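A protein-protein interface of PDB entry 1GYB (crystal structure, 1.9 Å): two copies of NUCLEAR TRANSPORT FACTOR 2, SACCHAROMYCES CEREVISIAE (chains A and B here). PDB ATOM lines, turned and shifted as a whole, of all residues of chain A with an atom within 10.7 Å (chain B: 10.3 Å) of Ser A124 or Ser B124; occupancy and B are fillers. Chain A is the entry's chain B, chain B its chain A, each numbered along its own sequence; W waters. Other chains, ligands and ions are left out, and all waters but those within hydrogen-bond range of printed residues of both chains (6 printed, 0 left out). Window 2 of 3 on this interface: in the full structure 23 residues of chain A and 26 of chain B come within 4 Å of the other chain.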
ATOM      1  N   GLU A  40      -7.907  27.374  31.797  1.00  0.00           N
ATOM      2  CA  GLU A  40      -8.415  26.191  32.490  1.00  0.00           C
ATOM      3  C   GLU A  40      -7.808  26.097  33.892  1.00  0.00           C
ATOM      4  O   GLU A  40      -7.248  25.068  34.288  1.00  0.00           O
ATOM      5  CB  GLU A  40      -8.134  24.921  31.678  1.00  0.00           C
ATOM      6  CG  GLU A  40      -9.139  24.681  30.553  1.00  0.00           C
ATOM      7  CD  GLU A  40     -10.554  24.418  31.062  1.00  0.00           C
ATOM      8  OE1 GLU A  40     -11.518  24.640  30.294  1.00  0.00           O
ATOM      9  OE2 GLU A  40     -10.712  23.984  32.230  1.00  0.00           O
ATOM     10  N   ARG A  65     -12.729  29.597  15.293  1.00  0.00           N
ATOM     11  CA  ARG A  65     -13.950  29.952  14.564  1.00  0.00           C
ATOM     12  C   ARG A  65     -14.801  30.701  15.588  1.00  0.00           C
ATOM     13  O   ARG A  65     -15.223  30.115  16.582  1.00  0.00           O
ATOM     14  CB  ARG A  65     -14.706  28.702  14.080  1.00  0.00           C
ATOM     15  CG  ARG A  65     -13.985  27.909  13.000  1.00  0.00           C
ATOM     16  CD  ARG A  65     -14.935  27.034  12.157  1.00  0.00           C
ATOM     17  NE  ARG A  65     -15.314  25.767  12.782  1.00  0.00           N
ATOM     18  CZ  ARG A  65     -16.416  25.575  13.505  1.00  0.00           C
ATOM     19  NH1 ARG A  65     -17.266  26.572  13.703  1.00  0.00           N
ATOM     20  NH2 ARG A  65     -16.674  24.380  14.023  1.00  0.00           N
ATOM     21  N   THR A  67     -18.037  32.374  17.179  1.00  0.00           N
ATOM     22  CA  THR A  67     -19.488  32.253  17.127  1.00  0.00           C
ATOM     23  C   THR A  67     -20.133  33.556  17.594  1.00  0.00           C
ATOM     24  O   THR A  67     -21.006  34.100  16.920  1.00  0.00           O
ATOM     25  CB  THR A  67     -19.982  31.105  18.011  1.00  0.00           C
ATOM     26  OG1 THR A  67     -19.339  29.890  17.605  1.00  0.00           O
ATOM     27  CG2 THR A  67     -21.488  30.947  17.880  1.00  0.00           C
ATOM     28  N   THR A  68     -19.710  34.047  18.756  1.00  0.00           N
ATOM     29  CA  THR A  68     -20.237  35.304  19.281  1.00  0.00           C
ATOM     30  C   THR A  68     -19.105  36.146  19.832  1.00  0.00           C
ATOM     31  O   THR A  68     -18.116  35.622  20.344  1.00  0.00           O
ATOM     32  CB  THR A  68     -21.273  35.097  20.427  1.00  0.00           C
ATOM     33  OG1 THR A  68     -20.666  34.374  21.506  1.00  0.00           O
ATOM     34  CG2 THR A  68     -22.488  34.341  19.924  1.00  0.00           C
ATOM     35  N   THR A  85     -17.181  33.522  22.352  1.00  0.00           N
ATOM     36  CA  THR A  85     -17.482  32.101  22.407  1.00  0.00           C
ATOM     37  C   THR A  85     -17.267  31.615  20.980  1.00  0.00           C
ATOM     38  O   THR A  85     -17.677  32.269  20.015  1.00  0.00           O
ATOM     39  CB  THR A  85     -18.914  31.805  22.870  1.00  0.00           C
ATOM     40  OG1 THR A  85     -18.984  31.974  24.289  1.00  0.00           O
ATOM     41  CG2 THR A  85     -19.300  30.365  22.527  1.00  0.00           C
ATOM     42  N   GLY A  86     -16.582  30.488  20.838  1.00  0.00           N
ATOM     43  CA  GLY A  86     -16.323  29.984  19.508  1.00  0.00           C
ATOM     44  C   GLY A  86     -15.835  28.553  19.534  1.00  0.00           C
ATOM     45  O   GLY A  86     -15.943  27.861  20.550  1.00  0.00           O
ATOM     46  N   ASP A  87     -15.286  28.122  18.406  1.00  0.00           N
ATOM     47  CA  ASP A  87     -14.786  26.768  18.257  1.00  0.00           C
ATOM     48  C   ASP A  87     -13.303  26.725  17.976  1.00  0.00           C
ATOM     49  O   ASP A  87     -12.754  27.580  17.277  1.00  0.00           O
ATOM     50  CB  ASP A  87     -15.503  26.063  17.107  1.00  0.00           C
ATOM     51  CG  ASP A  87     -16.923  25.704  17.443  1.00  0.00           C
ATOM     52  OD1 ASP A  87     -17.712  25.500  16.498  1.00  0.00           O
ATOM     53  OD2 ASP A  87     -17.247  25.615  18.648  1.00  0.00           O
ATOM     54  N   LEU A  88     -12.662  25.702  18.517  1.00  0.00           N
ATOM     55  CA  LEU A  88     -11.246  25.489  18.314  1.00  0.00           C
ATOM     56  C   LEU A  88     -11.157  24.220  17.466  1.00  0.00           C
ATOM     57  O   LEU A  88     -11.644  23.166  17.872  1.00  0.00           O
ATOM     58  CB  LEU A  88     -10.559  25.275  19.664  1.00  0.00           C
ATOM     59  CG  LEU A  88      -9.221  25.963  19.929  1.00  0.00           C
ATOM     60  CD1 LEU A  88      -9.359  27.465  19.713  1.00  0.00           C
ATOM     61  CD2 LEU A  88      -8.781  25.673  21.351  1.00  0.00           C
ATOM     62  N   GLN A  94     -12.448  17.883  12.050  1.00  0.00           N
ATOM     63  CA  GLN A  94     -13.734  18.524  11.834  1.00  0.00           C
ATOM     64  C   GLN A  94     -14.454  18.808  13.152  1.00  0.00           C
ATOM     65  O   GLN A  94     -14.975  19.906  13.353  1.00  0.00           O
ATOM     66  CB  GLN A  94     -14.611  17.648  10.934  1.00  0.00           C
ATOM     67  CG  GLN A  94     -14.110  17.507   9.489  1.00  0.00           C
ATOM     68  CD  GLN A  94     -14.992  16.579   8.673  1.00  0.00           C
ATOM     69  OE1 GLN A  94     -16.097  16.240   9.092  1.00  0.00           O
ATOM     70  NE2 GLN A  94     -14.514  16.170   7.503  1.00  0.00           N
ATOM     71  N   ASN A  95     -14.479  17.824  14.046  1.00  0.00           N
ATOM     72  CA  ASN A  95     -15.132  17.975  15.346  1.00  0.00           C
ATOM     73  C   ASN A  95     -14.526  19.148  16.118  1.00  0.00           C
ATOM     74  O   ASN A  95     -13.358  19.121  16.506  1.00  0.00           O
ATOM     75  CB  ASN A  95     -14.983  16.684  16.150  1.00  0.00           C
ATOM     76  CG  ASN A  95     -14.193  15.630  15.404  1.00  0.00           C
ATOM     77  OD1 ASN A  95     -13.021  15.830  15.079  1.00  0.00           O
ATOM     78  ND2 ASN A  95     -14.833  14.502  15.119  1.00  0.00           N
ATOM     79  N   PRO A  96     -15.326  20.197  16.354  1.00  0.00           N
ATOM     80  CA  PRO A  96     -14.896  21.397  17.074  1.00  0.00           C
ATOM     81  C   PRO A  96     -14.844  21.257  18.594  1.00  0.00           C
ATOM     82  O   PRO A  96     -15.569  20.463  19.187  1.00  0.00           O
ATOM     83  CB  PRO A  96     -15.924  22.429  16.637  1.00  0.00           C
ATOM     84  CG  PRO A  96     -17.167  21.613  16.574  1.00  0.00           C
ATOM     85  CD  PRO A  96     -16.707  20.357  15.860  1.00  0.00           C
ATOM     86  N   GLN A  97     -13.966  22.043  19.204  1.00  0.00           N
ATOM     87  CA  GLN A  97     -13.795  22.080  20.649  1.00  0.00           C
ATOM     88  C   GLN A  97     -14.238  23.490  21.027  1.00  0.00           C
ATOM     89  O   GLN A  97     -13.500  24.451  20.805  1.00  0.00           O
ATOM     90  CB  GLN A  97     -12.322  21.884  20.999  1.00  0.00           C
ATOM     91  CG  GLN A  97     -11.978  22.004  22.473  1.00  0.00           C
ATOM     92  CD  GLN A  97     -12.263  20.736  23.247  1.00  0.00           C
ATOM     93  OE1 GLN A  97     -13.412  20.332  23.394  1.00  0.00           O
ATOM     94  NE2 GLN A  97     -11.209  20.097  23.744  1.00  0.00           N
ATOM     95  N   ARG A  98     -15.443  23.617  21.572  1.00  0.00           N
ATOM     96  CA  ARG A  98     -15.966  24.926  21.940  1.00  0.00           C
ATOM     97  C   ARG A  98     -15.265  25.551  23.141  1.00  0.00           C
ATOM     98  O   ARG A  98     -14.834  24.854  24.068  1.00  0.00           O
ATOM     99  CB  ARG A  98     -17.469  24.844  22.203  1.00  0.00           C
ATOM    100  CG  ARG A  98     -18.113  26.205  22.381  1.00  0.00           C
ATOM    101  CD  ARG A  98     -19.621  26.125  22.398  1.00  0.00           C
ATOM    102  NE  ARG A  98     -20.123  25.388  23.555  1.00  0.00           N
ATOM    103  CZ  ARG A  98     -21.411  25.271  23.854  1.00  0.00           C
ATOM    104  NH1 ARG A  98     -22.322  25.845  23.076  1.00  0.00           N
ATOM    105  NH2 ARG A  98     -21.789  24.582  24.923  1.00  0.00           N
ATOM    106  N   PHE A  99     -15.171  26.879  23.120  1.00  0.00           N
ATOM    107  CA  PHE A  99     -14.506  27.615  24.186  1.00  0.00           C
ATOM    108  C   PHE A  99     -15.161  28.978  24.423  1.00  0.00           C
ATOM    109  O   PHE A  99     -15.929  29.469  23.589  1.00  0.00           O
ATOM    110  CB  PHE A  99     -13.036  27.830  23.809  1.00  0.00           C
ATOM    111  CG  PHE A  99     -12.836  28.889  22.758  1.00  0.00           C
ATOM    112  CD1 PHE A  99     -12.677  30.226  23.121  1.00  0.00           C
ATOM    113  CD2 PHE A  99     -12.858  28.562  21.403  1.00  0.00           C
ATOM    114  CE1 PHE A  99     -12.546  31.221  22.151  1.00  0.00           C
ATOM    115  CE2 PHE A  99     -12.728  29.550  20.422  1.00  0.00           C
ATOM    116  CZ  PHE A  99     -12.571  30.883  20.797  1.00  0.00           C
ATOM    117  N   SER A 100     -14.865  29.569  25.579  1.00  0.00           N
ATOM    118  CA  SER A 100     -15.351  30.902  25.927  1.00  0.00           C
ATOM    119  C   SER A 100     -14.102  31.648  26.379  1.00  0.00           C
ATOM    120  O   SER A 100     -13.260  31.087  27.084  1.00  0.00           O
ATOM    121  CB  SER A 100     -16.387  30.853  27.058  1.00  0.00           C
ATOM    122  OG  SER A 100     -17.634  30.373  26.584  1.00  0.00           O
ATOM    123  N   ARG A 120     -11.607  29.252  28.887  1.00  0.00           N
ATOM    124  CA  ARG A 120     -12.251  28.036  29.364  1.00  0.00           C
ATOM    125  C   ARG A 120     -12.796  27.217  28.210  1.00  0.00           C
ATOM    126  O   ARG A 120     -13.357  27.761  27.257  1.00  0.00           O
ATOM    127  CB  ARG A 120     -13.427  28.366  30.291  1.00  0.00           C
ATOM    128  CG  ARG A 120     -13.056  28.764  31.700  1.00  0.00           C
ATOM    129  CD  ARG A 120     -12.571  27.569  32.499  1.00  0.00           C
ATOM    130  NE  ARG A 120     -12.472  27.889  33.919  1.00  0.00           N
ATOM    131  CZ  ARG A 120     -12.137  27.018  34.863  1.00  0.00           C
ATOM    132  NH1 ARG A 120     -11.865  25.761  34.541  1.00  0.00           N
ATOM    133  NH2 ARG A 120     -12.087  27.402  36.131  1.00  0.00           N
ATOM    134  N   LEU A 121     -12.613  25.906  28.284  1.00  0.00           N
ATOM    135  CA  LEU A 121     -13.189  25.031  27.287  1.00  0.00           C
ATOM    136  C   LEU A 121     -14.664  25.090  27.692  1.00  0.00           C
ATOM    137  O   LEU A 121     -14.978  25.342  28.860  1.00  0.00           O
ATOM    138  CB  LEU A 121     -12.648  23.607  27.445  1.00  0.00           C
ATOM    139  CG  LEU A 121     -11.162  23.443  27.131  1.00  0.00           C
ATOM    140  CD1 LEU A 121     -10.751  21.986  27.363  1.00  0.00           C
ATOM    141  CD2 LEU A 121     -10.887  23.863  25.682  1.00  0.00           C
ATOM    142  N   ASN A 122     -15.569  24.862  26.752  1.00  0.00           N
ATOM    143  CA  ASN A 122     -16.997  24.937  27.052  1.00  0.00           C
ATOM    144  C   ASN A 122     -17.679  23.792  26.310  1.00  0.00           C
ATOM    145  O   ASN A 122     -18.183  23.969  25.197  1.00  0.00           O
ATOM    146  CB  ASN A 122     -17.524  26.303  26.580  1.00  0.00           C
ATOM    147  CG  ASN A 122     -18.910  26.630  27.114  1.00  0.00           C
ATOM    148  OD1 ASN A 122     -19.371  27.771  27.004  1.00  0.00           O
ATOM    149  ND2 ASN A 122     -19.581  25.643  27.681  1.00  0.00           N
ATOM    150  N   TYR A 123     -17.686  22.617  26.940  1.00  0.00           N
ATOM    151  CA  TYR A 123     -18.262  21.412  26.351  1.00  0.00           C
ATOM    152  C   TYR A 123     -19.563  21.602  25.578  1.00  0.00           C
ATOM    153  O   TYR A 123     -20.502  22.240  26.052  1.00  0.00           O
ATOM    154  CB  TYR A 123     -18.473  20.342  27.432  1.00  0.00           C
ATOM    155  CG  TYR A 123     -19.091  19.070  26.893  1.00  0.00           C
ATOM    156  CD1 TYR A 123     -18.398  18.262  25.992  1.00  0.00           C
ATOM    157  CD2 TYR A 123     -20.396  18.711  27.230  1.00  0.00           C
ATOM    158  CE1 TYR A 123     -18.994  17.131  25.429  1.00  0.00           C
ATOM    159  CE2 TYR A 123     -21.002  17.584  26.673  1.00  0.00           C
ATOM    160  CZ  TYR A 123     -20.297  16.803  25.771  1.00  0.00           C
ATOM    161  OH  TYR A 123     -20.917  15.725  25.177  1.00  0.00           O
ATOM    162  N   SER A 124     -19.614  21.029  24.379  1.00  0.00           N
ATOM    163  CA  SER A 124     -20.808  21.116  23.551  1.00  0.00           C
ATOM    164  C   SER A 124     -21.475  19.748  23.466  1.00  0.00           C
ATOM    165  O   SER A 124     -22.578  19.587  24.033  1.00  0.00           O
ATOM    166  CB  SER A 124     -20.450  21.601  22.147  1.00  0.00           C
ATOM    167  OG  SER A 124     -21.584  21.537  21.298  1.00  0.00           O
ATOM    168  OXT SER A 124     -20.874  18.852  22.838  1.00  0.00           O
ATOM    169  N   THR B  67     -20.821  26.264  36.295  1.00  0.00           N
ATOM    170  CA  THR B  67     -19.946  25.139  36.002  1.00  0.00           C
ATOM    171  C   THR B  67     -18.477  25.582  36.013  1.00  0.00           C
ATOM    172  O   THR B  67     -17.589  24.773  36.249  1.00  0.00           O
ATOM    173  CB  THR B  67     -20.318  24.443  34.668  1.00  0.00           C
ATOM    174  OG1 THR B  67     -20.311  25.390  33.597  1.00  0.00           O
ATOM    175  CG2 THR B  67     -21.717  23.814  34.785  1.00  0.00           C
ATOM    176  N   ASP B  87     -25.050  26.468  33.395  1.00  0.00           N
ATOM    177  CA  ASP B  87     -26.332  26.023  32.876  1.00  0.00           C
ATOM    178  C   ASP B  87     -27.441  26.912  33.412  1.00  0.00           C
ATOM    179  O   ASP B  87     -27.444  27.274  34.588  1.00  0.00           O
ATOM    180  CB  ASP B  87     -26.596  24.575  33.311  1.00  0.00           C
ATOM    181  CG  ASP B  87     -25.585  23.597  32.739  1.00  0.00           C
ATOM    182  OD1 ASP B  87     -25.537  22.447  33.223  1.00  0.00           O
ATOM    183  OD2 ASP B  87     -24.841  23.968  31.802  1.00  0.00           O
ATOM    184  N   PRO B  96     -31.220  22.221  30.374  1.00  0.00           N
ATOM    185  CA  PRO B  96     -30.739  23.589  30.574  1.00  0.00           C
ATOM    186  C   PRO B  96     -30.087  24.201  29.343  1.00  0.00           C
ATOM    187  O   PRO B  96     -29.688  23.498  28.409  1.00  0.00           O
ATOM    188  CB  PRO B  96     -29.744  23.433  31.716  1.00  0.00           C
ATOM    189  CG  PRO B  96     -29.147  22.082  31.431  1.00  0.00           C
ATOM    190  CD  PRO B  96     -30.379  21.256  31.106  1.00  0.00           C
ATOM    191  N   GLN B  97     -29.992  25.524  29.355  1.00  0.00           N
ATOM    192  CA  GLN B  97     -29.355  26.272  28.283  1.00  0.00           C
ATOM    193  C   GLN B  97     -27.966  26.660  28.781  1.00  0.00           C
ATOM    194  O   GLN B  97     -27.787  26.899  29.971  1.00  0.00           O
ATOM    195  CB  GLN B  97     -30.168  27.527  27.963  1.00  0.00           C
ATOM    196  CG  GLN B  97     -31.302  27.259  26.989  1.00  0.00           C
ATOM    197  CD  GLN B  97     -30.774  26.725  25.677  1.00  0.00           C
ATOM    198  OE1 GLN B  97     -31.409  25.894  25.030  1.00  0.00           O
ATOM    199  NE2 GLN B  97     -29.602  27.205  25.276  1.00  0.00           N
ATOM    200  N   ARG B  98     -26.980  26.691  27.889  1.00  0.00           N
ATOM    201  CA  ARG B  98     -25.632  27.078  28.293  1.00  0.00           C
ATOM    202  C   ARG B  98     -25.518  28.597  28.240  1.00  0.00           C
ATOM    203  O   ARG B  98     -26.027  29.231  27.312  1.00  0.00           O
ATOM    204  CB  ARG B  98     -24.579  26.461  27.365  1.00  0.00           C
ATOM    205  CG  ARG B  98     -24.369  24.961  27.566  1.00  0.00           C
ATOM    206  CD  ARG B  98     -23.804  24.658  28.960  1.00  0.00           C
ATOM    207  NE  ARG B  98     -22.446  25.164  29.137  1.00  0.00           N
ATOM    208  CZ  ARG B  98     -21.785  25.171  30.293  1.00  0.00           C
ATOM    209  NH1 ARG B  98     -22.355  24.695  31.397  1.00  0.00           N
ATOM    210  NH2 ARG B  98     -20.548  25.654  30.347  1.00  0.00           N
ATOM    211  N   PHE B  99     -24.859  29.178  29.237  1.00  0.00           N
ATOM    212  CA  PHE B  99     -24.668  30.621  29.261  1.00  0.00           C
ATOM    213  C   PHE B  99     -23.225  30.969  29.636  1.00  0.00           C
ATOM    214  O   PHE B  99     -22.511  30.166  30.236  1.00  0.00           O
ATOM    215  CB  PHE B  99     -25.644  31.267  30.251  1.00  0.00           C
ATOM    216  CG  PHE B  99     -25.203  31.190  31.687  1.00  0.00           C
ATOM    217  CD1 PHE B  99     -24.343  32.150  32.214  1.00  0.00           C
ATOM    218  CD2 PHE B  99     -25.637  30.153  32.507  1.00  0.00           C
ATOM    219  CE1 PHE B  99     -23.917  32.080  33.549  1.00  0.00           C
ATOM    220  CE2 PHE B  99     -25.219  30.071  33.841  1.00  0.00           C
ATOM    221  CZ  PHE B  99     -24.358  31.039  34.360  1.00  0.00           C
ATOM    222  N   LEU B 121     -26.263  33.433  25.769  1.00  0.00           N
ATOM    223  CA  LEU B 121     -26.659  32.035  25.828  1.00  0.00           C
ATOM    224  C   LEU B 121     -25.849  31.450  24.672  1.00  0.00           C
ATOM    225  O   LEU B 121     -25.747  32.070  23.608  1.00  0.00           O
ATOM    226  CB  LEU B 121     -28.158  31.854  25.574  1.00  0.00           C
ATOM    227  CG  LEU B 121     -29.092  32.223  26.728  1.00  0.00           C
ATOM    228  CD1 LEU B 121     -30.530  31.823  26.385  1.00  0.00           C
ATOM    229  CD2 LEU B 121     -28.641  31.500  27.993  1.00  0.00           C
ATOM    230  N   ASN B 122     -25.254  30.282  24.886  1.00  0.00           N
ATOM    231  CA  ASN B 122     -24.424  29.635  23.866  1.00  0.00           C
ATOM    232  C   ASN B 122     -25.122  28.414  23.297  1.00  0.00           C
ATOM    233  O   ASN B 122     -25.523  27.524  24.041  1.00  0.00           O
ATOM    234  CB  ASN B 122     -23.088  29.231  24.486  1.00  0.00           C
ATOM    235  CG  ASN B 122     -22.453  30.364  25.273  1.00  0.00           C
ATOM    236  OD1 ASN B 122     -22.124  31.409  24.712  1.00  0.00           O
ATOM    237  ND2 ASN B 122     -22.283  30.165  26.578  1.00  0.00           N
ATOM    238  N   TYR B 123     -25.258  28.363  21.977  1.00  0.00           N
ATOM    239  CA  TYR B 123     -25.941  27.240  21.343  1.00  0.00           C
ATOM    240  C   TYR B 123     -25.034  26.292  20.575  1.00  0.00           C
ATOM    241  O   TYR B 123     -24.090  26.721  19.909  1.00  0.00           O
ATOM    242  CB  TYR B 123     -27.029  27.760  20.405  1.00  0.00           C
ATOM    243  CG  TYR B 123     -28.053  28.615  21.103  1.00  0.00           C
ATOM    244  CD1 TYR B 123     -27.928  30.004  21.131  1.00  0.00           C
ATOM    245  CD2 TYR B 123     -29.140  28.033  21.753  1.00  0.00           C
ATOM    246  CE1 TYR B 123     -28.865  30.793  21.788  1.00  0.00           C
ATOM    247  CE2 TYR B 123     -30.079  28.809  22.415  1.00  0.00           C
ATOM    248  CZ  TYR B 123     -29.938  30.185  22.429  1.00  0.00           C
ATOM    249  OH  TYR B 123     -30.878  30.947  23.075  1.00  0.00           O
ATOM    250  N   SER B 124     -25.338  25.000  20.669  1.00  0.00           N
ATOM    251  CA  SER B 124     -24.566  23.973  19.978  1.00  0.00           C
ATOM    252  C   SER B 124     -24.964  23.879  18.510  1.00  0.00           C
ATOM    253  O   SER B 124     -24.056  23.835  17.655  1.00  0.00           O
ATOM    254  CB  SER B 124     -24.759  22.613  20.655  1.00  0.00           C
ATOM    255  OG  SER B 124     -24.058  22.557  21.888  1.00  0.00           O
ATOM    256  OXT SER B 124     -26.177  23.838  18.233  1.00  0.00           O
HETATM  257  O   HOH W   1     -21.018  22.404  28.670  1.00  0.00           O
HETATM  258  O   HOH W   2     -21.748  28.334  28.068  1.00  0.00           O
HETATM  259  O   HOH W   3     -21.637  28.154  20.549  1.00  0.00           O
HETATM  260  O   HOH W   4     -17.401  26.088  30.181  1.00  0.00           O
HETATM  261  O   HOH W   5     -24.528  24.603  24.163  1.00  0.00           O
HETATM  262  O   HOH W   6     -20.219  33.972  24.863  1.00  0.00           O
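OG of Ser A124 lies within hydrogen-bond range of OG of Ser B124 (2.7 Å).
The side-chain hydroxyl (OG1) of Thr A85 lies within hydrogen-bond range of the side-chain amide oxygen (OD1) of Asn B122, 3.2 Å away.
The side-chain amide nitrogen of Asn A122 sits close to the guanidinium group of Arg B98, at 2.8 Å.
OG of Ser A100 lies within hydrogen-bond range of OD1 of Asn A122 (3.2 Å).
O of Arg B98 is in hydrogen-bond range of N of Asn B122 (2.8 Å).
O of Arg A98 sits at hydrogen-bond distance from N of Asn A122, at 2.8 Å.
OG1 of Thr B67 lies within hydrogen-bond range of NH1 of Arg B98, at 3.1 Å.
The backbone NH (N) of Thr A67 sits at hydrogen-bond distance from the backbone carbonyl oxygen (O) of Thr A85 (2.9 Å).
OD2 of Asp B87 lies within salt-bridge range of NH1 of Arg B98 (2.6 Å).
NH2 of Arg A98 touches CG of Arg B98, at 3.7 Å.
Arg A98 touches Asn B122.
NH1 of Arg A98 touches C of Tyr B123, 3.7 Å away.
Arg A98 touches Ser B124 (NH1 to OG, 3.9 Å).
Asn B122 touches Asn A122 (ND2 to OD1, 3.8 Å).
Of the printed residues of chain B, Thr A85 touches Asn B122.
Printed residues of chain B within 4 Å of Arg A98: Arg B98, Asn B122, Tyr B123 and Ser B124.
Ser A124 touches just one residue of chain B: Ser B124.
Printed residues of chain A within 4 Å of Arg B98: Arg A98 and Asn A122.
Phe B99 touches none of the printed residues of chain A.
Leu B121 touches none of the printed residues of chain A.
Of chain A, only Arg A98 and Ser A124 come within 4 Å of Ser B124.
The nearest residue of chain B that does not touch Ser A124 is Tyr B123 (5.9 Å).
The nearest printed residue of chain B that does not touch Thr A85 is Tyr B123 (6.3 Å).
Of the 10 printed residues of chain B, 4 touch a printed residue of chain A.
Of the 20 printed residues of chain A, 4 touch a printed residue of chain B.
Printed residues of chain A that touch a printed residue of chain B: Thr A85, Arg A98, Asn A122 and Ser A124.
Along chain A the printed residues that touch a printed residue of chain B span positions 85 to 124.
Among the printed residues, 8 pairs touch across the chains.
Among the printed residues, no Asp or Glu carboxylate lies within 4 Å of a Lys or Arg side-chain nitrogen of the other chain.
Arg B98 touches its own counterpart, Arg A98.
Arg A98 touches Asn B122, and with the chains exchanged Asn A122 touches Arg B98.
Arg A98 touches Ser B124, but with the chains exchanged Ser A124 does not touch Arg B98 (6.6 Å).
Ser A124 touches its own counterpart, Ser B124.
Water W6 lies within hydrogen-bond range of OG1 of Thr A85 (2.4 Å), OD1 of Asn B122 (3.2 Å) and OG1 of Thr A68 (3.4 Å).
Water W2 lies within hydrogen-bond range of the side-chain amide nitrogen (ND2) of Asn B122 (2.4 Å), the side-chain amide oxygen (OD1) of Asn A122 (2.7 Å), the backbone carbonyl oxygen (O) of Phe B99 (2.9 Å) and the guanidinium group (NE) of Arg B98 (3.4 Å).
Water W1 bridges O of Tyr A123 and NE of Arg B98.
Water W5 lies within hydrogen-bond range of NH1 of Arg A98 (2.8 Å), O of Asn B122 (3.1 Å) and OG of Ser B124 (3.1 Å).
Water W4 lies within hydrogen-bond range of O of Leu A121 (2.9 Å), NH2 of Arg B98 (3.2 Å) and ND2 of Asn A122 (3.3 Å).
Water W3 lies within hydrogen-bond range of the backbone carbonyl oxygen of Tyr B123 (2.9 Å) and the guanidinium group of Arg A98 (3.5 Å).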
